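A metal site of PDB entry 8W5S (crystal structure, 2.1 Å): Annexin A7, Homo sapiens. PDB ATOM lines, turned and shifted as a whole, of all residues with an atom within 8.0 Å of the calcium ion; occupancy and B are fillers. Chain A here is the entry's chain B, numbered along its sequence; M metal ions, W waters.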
ATOM      1  N   SER A 206      29.907  19.444  18.176  1.00  0.00           N
ATOM      2  CA  SER A 206      28.545  19.882  17.924  1.00  0.00           C
ATOM      3  C   SER A 206      28.288  21.259  18.529  1.00  0.00           C
ATOM      4  O   SER A 206      27.821  22.172  17.851  1.00  0.00           O
ATOM      5  CB  SER A 206      27.545  18.865  18.472  1.00  0.00           C
ATOM      6  OG  SER A 206      27.749  17.579  17.919  1.00  0.00           O
ATOM      7  N   SER A 207      28.605  21.414  19.826  1.00  0.00           N
ATOM      8  CA  SER A 207      28.379  22.686  20.504  1.00  0.00           C
ATOM      9  C   SER A 207      29.067  23.838  19.788  1.00  0.00           C
ATOM     10  O   SER A 207      28.516  24.941  19.710  1.00  0.00           O
ATOM     11  CB  SER A 207      28.870  22.598  21.953  1.00  0.00           C
ATOM     12  OG  SER A 207      28.398  21.421  22.579  1.00  0.00           O
ATOM     13  N   VAL A 208      30.259  23.592  19.236  1.00  0.00           N
ATOM     14  CA  VAL A 208      30.951  24.634  18.490  1.00  0.00           C
ATOM     15  C   VAL A 208      30.190  24.972  17.209  1.00  0.00           C
ATOM     16  O   VAL A 208      30.000  26.146  16.877  1.00  0.00           O
ATOM     17  CB  VAL A 208      32.397  24.209  18.196  1.00  0.00           C
ATOM     18  CG1 VAL A 208      33.061  25.196  17.236  1.00  0.00           C
ATOM     19  CG2 VAL A 208      33.197  24.099  19.486  1.00  0.00           C
ATOM     20  N   SER A 209      29.739  23.951  16.489  1.00  0.00           N
ATOM     21  CA  SER A 209      28.884  24.185  15.333  1.00  0.00           C
ATOM     22  C   SER A 209      27.601  24.905  15.731  1.00  0.00           C
ATOM     23  O   SER A 209      27.114  25.774  15.011  1.00  0.00           O
ATOM     24  CB  SER A 209      28.560  22.864  14.628  1.00  0.00           C
ATOM     25  OG  SER A 209      29.569  21.890  14.874  1.00  0.00           O
ATOM     26  N   ARG A 210      27.054  24.548  16.898  1.00  0.00           N
ATOM     27  CA  ARG A 210      25.804  25.142  17.346  1.00  0.00           C
ATOM     28  C   ARG A 210      25.993  26.554  17.903  1.00  0.00           C
ATOM     29  O   ARG A 210      25.092  27.384  17.754  1.00  0.00           O
ATOM     30  CB  ARG A 210      25.158  24.241  18.407  1.00  0.00           C
ATOM     31  CG  ARG A 210      24.353  23.089  17.815  1.00  0.00           C
ATOM     32  CD  ARG A 210      24.568  21.797  18.581  1.00  0.00           C
ATOM     33  NE  ARG A 210      24.110  21.862  19.962  1.00  0.00           N
ATOM     34  CZ  ARG A 210      22.838  21.925  20.342  1.00  0.00           C
ATOM     35  NH1 ARG A 210      21.855  21.958  19.456  1.00  0.00           N
ATOM     36  NH2 ARG A 210      22.543  21.959  21.643  1.00  0.00           N
ATOM     37  N   GLU A 211      27.133  26.840  18.517  1.00  0.00           N
ATOM     38  CA  GLU A 211      27.360  28.125  19.167  1.00  0.00           C
ATOM     39  C   GLU A 211      28.147  29.118  18.325  1.00  0.00           C
ATOM     40  O   GLU A 211      28.161  30.303  18.662  1.00  0.00           O
ATOM     41  CB  GLU A 211      28.071  27.925  20.505  1.00  0.00           C
ATOM     42  CG  GLU A 211      27.243  27.196  21.536  1.00  0.00           C
ATOM     43  CD  GLU A 211      26.157  28.069  22.129  1.00  0.00           C
ATOM     44  OE1 GLU A 211      26.350  29.301  22.180  1.00  0.00           O
ATOM     45  OE2 GLU A 211      25.118  27.522  22.550  1.00  0.00           O
ATOM     46  N   PHE A 212      28.801  28.675  17.258  1.00  0.00           N
ATOM     47  CA  PHE A 212      29.573  29.570  16.407  1.00  0.00           C
ATOM     48  C   PHE A 212      29.105  29.461  14.965  1.00  0.00           C
ATOM     49  O   PHE A 212      28.437  28.499  14.580  1.00  0.00           O
ATOM     50  CB  PHE A 212      31.074  29.249  16.476  1.00  0.00           C
ATOM     51  CG  PHE A 212      31.692  29.507  17.809  1.00  0.00           C
ATOM     52  CD1 PHE A 212      32.191  30.756  18.131  1.00  0.00           C
ATOM     53  CD2 PHE A 212      31.787  28.495  18.744  1.00  0.00           C
ATOM     54  CE1 PHE A 212      32.763  31.000  19.359  1.00  0.00           C
ATOM     55  CE2 PHE A 212      32.363  28.725  19.985  1.00  0.00           C
ATOM     56  CZ  PHE A 212      32.848  29.984  20.293  1.00  0.00           C
ATOM     57  N   SER A 213      29.454  30.475  14.185  1.00  0.00           N
ATOM     58  CA  SER A 213      29.321  30.423  12.736  1.00  0.00           C
ATOM     59  C   SER A 213      30.583  30.971  12.087  1.00  0.00           C
ATOM     60  O   SER A 213      31.599  31.166  12.774  1.00  0.00           O
ATOM     61  CB  SER A 213      28.104  31.227  12.264  1.00  0.00           C
ATOM     62  OG  SER A 213      28.432  32.590  12.118  1.00  0.00           O
ATOM     63  N   GLY A 214      30.563  31.193  10.778  1.00  0.00           N
ATOM     64  CA  GLY A 214      31.654  31.857  10.094  1.00  0.00           C
ATOM     65  C   GLY A 214      32.966  31.102  10.173  1.00  0.00           C
ATOM     66  O   GLY A 214      33.016  29.873  10.337  1.00  0.00           O
ATOM     67  N   GLU A 217      34.164  29.307  13.545  1.00  0.00           N
ATOM     68  CA  GLU A 217      33.746  27.918  13.631  1.00  0.00           C
ATOM     69  C   GLU A 217      34.733  27.004  12.918  1.00  0.00           C
ATOM     70  O   GLU A 217      35.171  25.986  13.464  1.00  0.00           O
ATOM     71  CB  GLU A 217      32.342  27.769  13.047  1.00  0.00           C
ATOM     72  CG  GLU A 217      31.854  26.326  12.902  1.00  0.00           C
ATOM     73  CD  GLU A 217      30.384  26.247  12.545  1.00  0.00           C
ATOM     74  OE1 GLU A 217      29.761  27.309  12.385  1.00  0.00           O
ATOM     75  OE2 GLU A 217      29.856  25.121  12.423  1.00  0.00           O
ATOM     76  N   LYS A 221      36.897  24.344  14.995  1.00  0.00           N
ATOM     77  CA  LYS A 221      36.637  22.936  14.731  1.00  0.00           C
ATOM     78  C   LYS A 221      37.856  22.254  14.123  1.00  0.00           C
ATOM     79  O   LYS A 221      38.014  21.030  14.262  1.00  0.00           O
ATOM     80  CB  LYS A 221      35.418  22.777  13.828  1.00  0.00           C
ATOM     81  CG  LYS A 221      34.118  23.243  14.467  1.00  0.00           C
ATOM     82  CD  LYS A 221      32.996  22.242  14.294  1.00  0.00           C
ATOM     83  CE  LYS A 221      32.624  22.058  12.833  1.00  0.00           C
ATOM     84  NZ  LYS A 221      31.660  23.091  12.382  1.00  0.00           N
HETATM   85 CA    CA M   1      27.120  27.280  13.201  1.00  0.00          CA
HETATM   86  O   HOH W   1      26.942  24.610  11.819  1.00  0.00           O
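O of Phe 212 is bound to the calcium ion, at 2.3 Å. O of Ser 209 binds the calcium ion (2.4 Å). OE1 of Glu 217 is bound to the calcium ion, 2.8 Å away. The calcium ion has three donor atoms within binding distance. Slightly farther from the calcium ion lies water W1 (3.0 Å).
Merely in contact with the calcium ion: Ser 213. The nearest printed residue that does not touch the calcium ion is Arg 210 (4.6 Å).
OG of Ser 209 sits close to O of Ser 206. NZ of Lys 221 lies within salt-bridge range of OE2 of Glu 217 (2.7 Å). OG of Ser 209 sits at hydrogen-bond distance from NZ of Lys 221 (3.5 Å).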
